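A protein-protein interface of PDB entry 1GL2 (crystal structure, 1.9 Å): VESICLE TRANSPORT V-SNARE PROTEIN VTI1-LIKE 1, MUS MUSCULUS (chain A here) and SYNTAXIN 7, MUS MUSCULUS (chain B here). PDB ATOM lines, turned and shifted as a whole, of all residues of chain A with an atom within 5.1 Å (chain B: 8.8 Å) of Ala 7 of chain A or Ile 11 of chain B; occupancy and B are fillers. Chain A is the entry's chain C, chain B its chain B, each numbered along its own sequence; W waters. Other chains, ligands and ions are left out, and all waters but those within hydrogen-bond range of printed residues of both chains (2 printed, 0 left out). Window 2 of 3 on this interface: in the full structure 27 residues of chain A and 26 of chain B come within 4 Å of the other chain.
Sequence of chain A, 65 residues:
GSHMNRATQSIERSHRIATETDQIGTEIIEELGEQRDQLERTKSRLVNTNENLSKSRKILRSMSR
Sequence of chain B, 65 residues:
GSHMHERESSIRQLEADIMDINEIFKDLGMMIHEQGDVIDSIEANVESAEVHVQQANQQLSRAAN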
ATOM      1  N   ASN A   5     -16.899  -5.987   9.168  1.00  0.00           N
ATOM      2  CA  ASN A   5     -17.878  -6.751   9.923  1.00  0.00           C
ATOM      3  C   ASN A   5     -17.196  -7.621  10.971  1.00  0.00           C
ATOM      4  O   ASN A   5     -15.975  -7.579  11.131  1.00  0.00           O
ATOM      5  CB  ASN A   5     -18.693  -7.627   8.976  1.00  0.00           C
ATOM      6  CG  ASN A   5     -17.820  -8.469   8.067  1.00  0.00           C
ATOM      7  OD1 ASN A   5     -17.010  -9.266   8.531  1.00  0.00           O
ATOM      8  ND2 ASN A   5     -17.981  -8.292   6.766  1.00  0.00           N
ATOM      9  N   ARG A   6     -17.993  -8.418  11.675  1.00  0.00           N
ATOM     10  CA  ARG A   6     -17.472  -9.297  12.714  1.00  0.00           C
ATOM     11  C   ARG A   6     -16.354 -10.209  12.204  1.00  0.00           C
ATOM     12  O   ARG A   6     -15.396 -10.487  12.928  1.00  0.00           O
ATOM     13  CB  ARG A   6     -18.612 -10.142  13.297  1.00  0.00           C
ATOM     14  CG  ARG A   6     -19.668  -9.350  14.093  1.00  0.00           C
ATOM     15  CD  ARG A   6     -19.123  -8.888  15.439  1.00  0.00           C
ATOM     16  NE  ARG A   6     -20.180  -8.564  16.396  1.00  0.00           N
ATOM     17  CZ  ARG A   6     -20.688  -7.348  16.590  1.00  0.00           C
ATOM     18  NH1 ARG A   6     -21.651  -7.164  17.488  1.00  0.00           N
ATOM     19  NH2 ARG A   6     -20.233  -6.311  15.900  1.00  0.00           N
ATOM     20  N   ALA A   7     -16.470 -10.665  10.959  1.00  0.00           N
ATOM     21  CA  ALA A   7     -15.470 -11.557  10.373  1.00  0.00           C
ATOM     22  C   ALA A   7     -14.131 -10.863  10.103  1.00  0.00           C
ATOM     23  O   ALA A   7     -13.078 -11.360  10.499  1.00  0.00           O
ATOM     24  CB  ALA A   7     -16.010 -12.170   9.082  1.00  0.00           C
ATOM     25  N   THR A   8     -14.174  -9.715   9.434  1.00  0.00           N
ATOM     26  CA  THR A   8     -12.954  -8.987   9.118  1.00  0.00           C
ATOM     27  C   THR A   8     -12.192  -8.599  10.380  1.00  0.00           C
ATOM     28  O   THR A   8     -10.970  -8.749  10.440  1.00  0.00           O
ATOM     29  CB  THR A   8     -13.248  -7.711   8.272  1.00  0.00           C
ATOM     30  OG1 THR A   8     -14.087  -6.811   9.005  1.00  0.00           O
ATOM     31  CG2 THR A   8     -13.947  -8.085   6.974  1.00  0.00           C
ATOM     32  N   GLN A   9     -12.910  -8.108  11.391  1.00  0.00           N
ATOM     33  CA  GLN A   9     -12.276  -7.700  12.639  1.00  0.00           C
ATOM     34  C   GLN A   9     -11.724  -8.895  13.415  1.00  0.00           C
ATOM     35  O   GLN A   9     -10.671  -8.801  14.045  1.00  0.00           O
ATOM     36  CB  GLN A   9     -13.269  -6.902  13.489  1.00  0.00           C
ATOM     37  CG  GLN A   9     -13.750  -5.647  12.774  1.00  0.00           C
ATOM     38  CD  GLN A   9     -12.596  -4.891  12.131  1.00  0.00           C
ATOM     39  OE1 GLN A   9     -11.766  -4.307  12.822  1.00  0.00           O
ATOM     40  NE2 GLN A   9     -12.528  -4.921  10.800  1.00  0.00           N
ATOM     41  N   SER A  10     -12.425 -10.023  13.357  1.00  0.00           N
ATOM     42  CA  SER A  10     -11.954 -11.219  14.041  1.00  0.00           C
ATOM     43  C   SER A  10     -10.663 -11.710  13.369  1.00  0.00           C
ATOM     44  O   SER A  10      -9.714 -12.092  14.046  1.00  0.00           O
ATOM     45  CB  SER A  10     -13.022 -12.318  13.995  1.00  0.00           C
ATOM     46  OG  SER A  10     -12.544 -13.518  14.585  1.00  0.00           O
ATOM     47  N   ILE A  11     -10.628 -11.697  12.039  1.00  0.00           N
ATOM     48  CA  ILE A  11      -9.435 -12.130  11.306  1.00  0.00           C
ATOM     49  C   ILE A  11      -8.226 -11.272  11.671  1.00  0.00           C
ATOM     50  O   ILE A  11      -7.108 -11.773  11.803  1.00  0.00           O
ATOM     51  CB  ILE A  11      -9.655 -12.048   9.776  1.00  0.00           C
ATOM     52  CG1 ILE A  11     -10.673 -13.108   9.349  1.00  0.00           C
ATOM     53  CG2 ILE A  11      -8.333 -12.263   9.034  1.00  0.00           C
ATOM     54  CD1 ILE A  11     -11.086 -13.024   7.898  1.00  0.00           C
ATOM     55  N   GLU A  12      -8.458  -9.976  11.842  1.00  0.00           N
ATOM     56  CA  GLU A  12      -7.398  -9.044  12.191  1.00  0.00           C
ATOM     57  C   GLU A  12      -6.843  -9.343  13.579  1.00  0.00           C
ATOM     58  O   GLU A  12      -5.633  -9.315  13.786  1.00  0.00           O
ATOM     59  CB  GLU A  12      -7.927  -7.618  12.163  1.00  0.00           C
ATOM     60  CG  GLU A  12      -6.852  -6.576  12.091  1.00  0.00           C
ATOM     61  CD  GLU A  12      -7.415  -5.179  12.172  1.00  0.00           C
ATOM     62  OE1 GLU A  12      -7.602  -4.676  13.296  1.00  0.00           O
ATOM     63  OE2 GLU A  12      -7.692  -4.590  11.109  1.00  0.00           O
ATOM     64  N   HIS B   5     -24.290 -16.443   8.346  1.00  0.00           N
ATOM     65  CA  HIS B   5     -23.315 -16.228   9.452  1.00  0.00           C
ATOM     66  C   HIS B   5     -22.497 -17.475   9.793  1.00  0.00           C
ATOM     67  O   HIS B   5     -21.764 -17.478  10.778  1.00  0.00           O
ATOM     68  CB  HIS B   5     -24.038 -15.740  10.717  1.00  0.00           C
ATOM     69  CG  HIS B   5     -24.702 -14.406  10.564  1.00  0.00           C
ATOM     70  ND1 HIS B   5     -25.831 -14.217   9.795  1.00  0.00           N
ATOM     71  CD2 HIS B   5     -24.391 -13.189  11.076  1.00  0.00           C
ATOM     72  CE1 HIS B   5     -26.188 -12.946   9.838  1.00  0.00           C
ATOM     73  NE2 HIS B   5     -25.330 -12.300  10.608  1.00  0.00           N
ATOM     74  N   GLU B   6     -22.611 -18.532   8.993  1.00  0.00           N
ATOM     75  CA  GLU B   6     -21.845 -19.742   9.279  1.00  0.00           C
ATOM     76  C   GLU B   6     -20.362 -19.526   9.020  1.00  0.00           C
ATOM     77  O   GLU B   6     -19.519 -20.035   9.756  1.00  0.00           O
ATOM     78  CB  GLU B   6     -22.334 -20.939   8.457  1.00  0.00           C
ATOM     79  CG  GLU B   6     -21.436 -22.171   8.632  1.00  0.00           C
ATOM     80  CD  GLU B   6     -21.929 -23.397   7.872  1.00  0.00           C
ATOM     81  OE1 GLU B   6     -22.317 -23.255   6.689  1.00  0.00           O
ATOM     82  OE2 GLU B   6     -21.910 -24.507   8.457  1.00  0.00           O
ATOM     83  N   ARG B   7     -20.035 -18.786   7.966  1.00  0.00           N
ATOM     84  CA  ARG B   7     -18.633 -18.516   7.681  1.00  0.00           C
ATOM     85  C   ARG B   7     -18.132 -17.566   8.765  1.00  0.00           C
ATOM     86  O   ARG B   7     -17.035 -17.731   9.288  1.00  0.00           O
ATOM     87  CB  ARG B   7     -18.470 -17.885   6.303  1.00  0.00           C
ATOM     88  CG  ARG B   7     -17.022 -17.721   5.877  1.00  0.00           C
ATOM     89  CD  ARG B   7     -16.925 -17.618   4.367  1.00  0.00           C
ATOM     90  NE  ARG B   7     -15.566 -17.368   3.895  1.00  0.00           N
ATOM     91  CZ  ARG B   7     -14.910 -16.226   4.074  1.00  0.00           C
ATOM     92  NH1 ARG B   7     -13.678 -16.096   3.605  1.00  0.00           N
ATOM     93  NH2 ARG B   7     -15.482 -15.214   4.719  1.00  0.00           N
ATOM     94  N   GLU B   8     -18.946 -16.570   9.099  1.00  0.00           N
ATOM     95  CA  GLU B   8     -18.585 -15.628  10.147  1.00  0.00           C
ATOM     96  C   GLU B   8     -18.356 -16.414  11.435  1.00  0.00           C
ATOM     97  O   GLU B   8     -17.360 -16.210  12.127  1.00  0.00           O
ATOM     98  CB  GLU B   8     -19.699 -14.598  10.363  1.00  0.00           C
ATOM     99  CG  GLU B   8     -19.688 -13.989  11.763  1.00  0.00           C
ATOM    100  CD  GLU B   8     -20.713 -12.879  11.962  1.00  0.00           C
ATOM    101  OE1 GLU B   8     -21.237 -12.764  13.094  1.00  0.00           O
ATOM    102  OE2 GLU B   8     -20.981 -12.116  11.004  1.00  0.00           O
ATOM    103  N   SER B   9     -19.281 -17.316  11.747  1.00  0.00           N
ATOM    104  CA  SER B   9     -19.172 -18.134  12.950  1.00  0.00           C
ATOM    105  C   SER B   9     -17.891 -18.956  12.965  1.00  0.00           C
ATOM    106  O   SER B   9     -17.179 -18.994  13.973  1.00  0.00           O
ATOM    107  CB  SER B   9     -20.375 -19.070  13.071  1.00  0.00           C
ATOM    108  OG  SER B   9     -21.543 -18.334  13.370  1.00  0.00           O
ATOM    109  N   SER B  10     -17.604 -19.625  11.852  1.00  0.00           N
ATOM    110  CA  SER B  10     -16.402 -20.440  11.758  1.00  0.00           C
ATOM    111  C   SER B  10     -15.171 -19.572  11.966  1.00  0.00           C
ATOM    112  O   SER B  10     -14.209 -19.996  12.607  1.00  0.00           O
ATOM    113  CB  SER B  10     -16.328 -21.129  10.394  1.00  0.00           C
ATOM    114  OG  SER B  10     -17.354 -22.098  10.279  1.00  0.00           O
ATOM    115  N   ILE B  11     -15.211 -18.357  11.429  1.00  0.00           N
ATOM    116  CA  ILE B  11     -14.097 -17.425  11.557  1.00  0.00           C
ATOM    117  C   ILE B  11     -13.916 -16.971  13.010  1.00  0.00           C
ATOM    118  O   ILE B  11     -12.795 -16.926  13.519  1.00  0.00           O
ATOM    119  CB  ILE B  11     -14.311 -16.201  10.632  1.00  0.00           C
ATOM    120  CG1 ILE B  11     -14.171 -16.643   9.174  1.00  0.00           C
ATOM    121  CG2 ILE B  11     -13.320 -15.091  10.974  1.00  0.00           C
ATOM    122  CD1 ILE B  11     -14.427 -15.547   8.158  1.00  0.00           C
ATOM    123  N   ARG B  12     -15.022 -16.648  13.674  1.00  0.00           N
ATOM    124  CA  ARG B  12     -14.984 -16.208  15.066  1.00  0.00           C
ATOM    125  C   ARG B  12     -14.523 -17.333  15.998  1.00  0.00           C
ATOM    126  O   ARG B  12     -13.843 -17.088  16.995  1.00  0.00           O
ATOM    127  CB  ARG B  12     -16.368 -15.690  15.477  1.00  0.00           C
ATOM    128  CG  ARG B  12     -16.813 -14.488  14.639  1.00  0.00           C
ATOM    129  CD  ARG B  12     -18.269 -14.098  14.869  1.00  0.00           C
ATOM    130  NE  ARG B  12     -18.509 -13.674  16.246  1.00  0.00           N
ATOM    131  CZ  ARG B  12     -19.561 -12.963  16.637  1.00  0.00           C
ATOM    132  NH1 ARG B  12     -19.692 -12.625  17.912  1.00  0.00           N
ATOM    133  NH2 ARG B  12     -20.476 -12.588  15.755  1.00  0.00           N
ATOM    134  N   GLN B  13     -14.888 -18.569  15.672  1.00  0.00           N
ATOM    135  CA  GLN B  13     -14.484 -19.719  16.479  1.00  0.00           C
ATOM    136  C   GLN B  13     -13.004 -19.993  16.268  1.00  0.00           C
ATOM    137  O   GLN B  13     -12.298 -20.440  17.174  1.00  0.00           O
ATOM    138  CB  GLN B  13     -15.302 -20.949  16.093  1.00  0.00           C
ATOM    139  CG  GLN B  13     -16.738 -20.882  16.579  1.00  0.00           C
ATOM    140  CD  GLN B  13     -17.618 -21.910  15.904  1.00  0.00           C
ATOM    141  OE1 GLN B  13     -17.253 -23.082  15.803  1.00  0.00           O
ATOM    142  NE2 GLN B  13     -18.790 -21.478  15.440  1.00  0.00           N
ATOM    143  N   LEU B  14     -12.544 -19.714  15.058  1.00  0.00           N
ATOM    144  CA  LEU B  14     -11.150 -19.898  14.708  1.00  0.00           C
ATOM    145  C   LEU B  14     -10.311 -19.010  15.628  1.00  0.00           C
ATOM    146  O   LEU B  14      -9.235 -19.409  16.088  1.00  0.00           O
ATOM    147  CB  LEU B  14     -10.934 -19.483  13.253  1.00  0.00           C
ATOM    148  CG  LEU B  14      -9.545 -19.715  12.662  1.00  0.00           C
ATOM    149  CD1 LEU B  14      -9.315 -21.207  12.463  1.00  0.00           C
ATOM    150  CD2 LEU B  14      -9.438 -18.982  11.334  1.00  0.00           C
ATOM    151  N   GLU B  15     -10.817 -17.808  15.900  1.00  0.00           N
ATOM    152  CA  GLU B  15     -10.108 -16.858  16.753  1.00  0.00           C
ATOM    153  C   GLU B  15      -9.946 -17.399  18.160  1.00  0.00           C
ATOM    154  O   GLU B  15      -8.881 -17.272  18.757  1.00  0.00           O
ATOM    155  CB  GLU B  15     -10.852 -15.517  16.809  1.00  0.00           C
ATOM    156  CG  GLU B  15     -10.105 -14.419  17.571  1.00  0.00           C
ATOM    157  CD  GLU B  15     -10.930 -13.151  17.742  1.00  0.00           C
ATOM    158  OE1 GLU B  15     -12.018 -13.049  17.134  1.00  0.00           O
ATOM    159  OE2 GLU B  15     -10.486 -12.248  18.482  1.00  0.00           O
ATOM    160  N   ALA B  16     -11.008 -17.993  18.694  1.00  0.00           N
ATOM    161  CA  ALA B  16     -10.956 -18.550  20.042  1.00  0.00           C
ATOM    162  C   ALA B  16      -9.921 -19.660  20.102  1.00  0.00           C
ATOM    163  O   ALA B  16      -9.212 -19.797  21.093  1.00  0.00           O
ATOM    164  CB  ALA B  16     -12.331 -19.089  20.456  1.00  0.00           C
ATOM    165  N   ASP B  17      -9.846 -20.451  19.037  1.00  0.00           N
ATOM    166  CA  ASP B  17      -8.902 -21.558  18.956  1.00  0.00           C
ATOM    167  C   ASP B  17      -7.469 -21.046  18.827  1.00  0.00           C
ATOM    168  O   ASP B  17      -6.536 -21.671  19.322  1.00  0.00           O
ATOM    169  CB  ASP B  17      -9.257 -22.452  17.765  1.00  0.00           C
ATOM    170  CG  ASP B  17     -10.494 -23.303  18.018  1.00  0.00           C
ATOM    171  OD1 ASP B  17     -11.124 -23.731  17.034  1.00  0.00           O
ATOM    172  OD2 ASP B  17     -10.833 -23.558  19.194  1.00  0.00           O
ATOM    173  N   ILE B  18      -7.296 -19.917  18.149  1.00  0.00           N
ATOM    174  CA  ILE B  18      -5.973 -19.328  17.990  1.00  0.00           C
ATOM    175  C   ILE B  18      -5.523 -18.733  19.328  1.00  0.00           C
ATOM    176  O   ILE B  18      -4.335 -18.729  19.643  1.00  0.00           O
ATOM    177  CB  ILE B  18      -5.985 -18.246  16.879  1.00  0.00           C
ATOM    178  CG1 ILE B  18      -6.096 -18.933  15.510  1.00  0.00           C
ATOM    179  CG2 ILE B  18      -4.728 -17.373  16.952  1.00  0.00           C
ATOM    180  CD1 ILE B  18      -6.342 -17.991  14.353  1.00  0.00           C
HETATM  181  O   HOH W   1     -19.074 -11.025   9.426  1.00  0.00           O
HETATM  182  O   HOH W   2     -10.507 -15.179  13.246  1.00  0.00           O
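The side-chain carboxylate (OE1) of Glu 8 of chain B is in salt-bridge range of the guanidinium group (NH2) of Arg 12 of chain B.
The side-chain amide oxygen (OD1) of Asn 5 of chain A lies within hydrogen-bond range of the backbone NH (N) of Ala 7 of chain A (2.9 Å).
The side-chain carboxylate (OE1) of Glu 15 of chain B lies within hydrogen-bond range of the side-chain hydroxyl (OG) of Ser 10 of chain A (2.6 Å).
Water W1 lies within hydrogen-bond range of OE2 of Glu 8 of chain B, OD1 of Asn 5 of chain A and N of Ala 7 of chain A.
Water W2 lies within hydrogen-bond range of O of Ile 11 of chain B (2.9 Å) and OG of Ser 10 of chain A (2.9 Å).
Along chain B the printed residues that touch a printed residue of chain A span positions 8 to 15.
Among the printed residues, 7 pairs touch across the chains.
Among the printed residues, no Asp or Glu carboxylate lies within 4 Å of a Lys or Arg side-chain nitrogen of the other chain.
Of chain B, only Ile 11 comes within 4 Å of Ala 7 of chain A.
Printed residues of chain A within 4 Å of Ile 11 of chain B: Ala 7, Ser 10 and Ile 11.
No residue of chain B comes within 4 Å of Thr 8 of chain A.
Of the printed residues of chain A, Glu 8 of chain B touches Arg 6 (3.7 Å).
Printed residues of chain B within 4 Å of Ser 10 of chain A: Ile 11 (3.6 Å), Arg 12 (3.7 Å) and Glu 15 (2.6 Å).
Printed residues of chain A within 4 Å of Glu 15 of chain B: Ser 10.
Printed residues of chain A within 4 Å of Arg 12 of chain B: Arg 6 (3.7 Å) and Ser 10 (3.7 Å).
Leu 14 of chain B touches none of the printed residues of chain A.
The nearest residue of chain B that does not touch Ala 7 of chain A is Glu 8 of chain B (4.4 Å).
The nearest printed residue of chain A that does not touch Arg 12 of chain B is Ala 7 of chain A (5.3 Å).
Among the printed residues, merely in contact across the chains: Arg 6 of chain A with Glu 8 of chain B, Arg 6 of chain A with Arg 12 of chain B, Ala 7 of chain A with Ile 11 of chain B, Ser 10 of chain A with Ile 11 of chain B, Ser 10 of chain A with Arg 12 of chain B and Ile 11 of chain A with Ile 11 of chain B.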
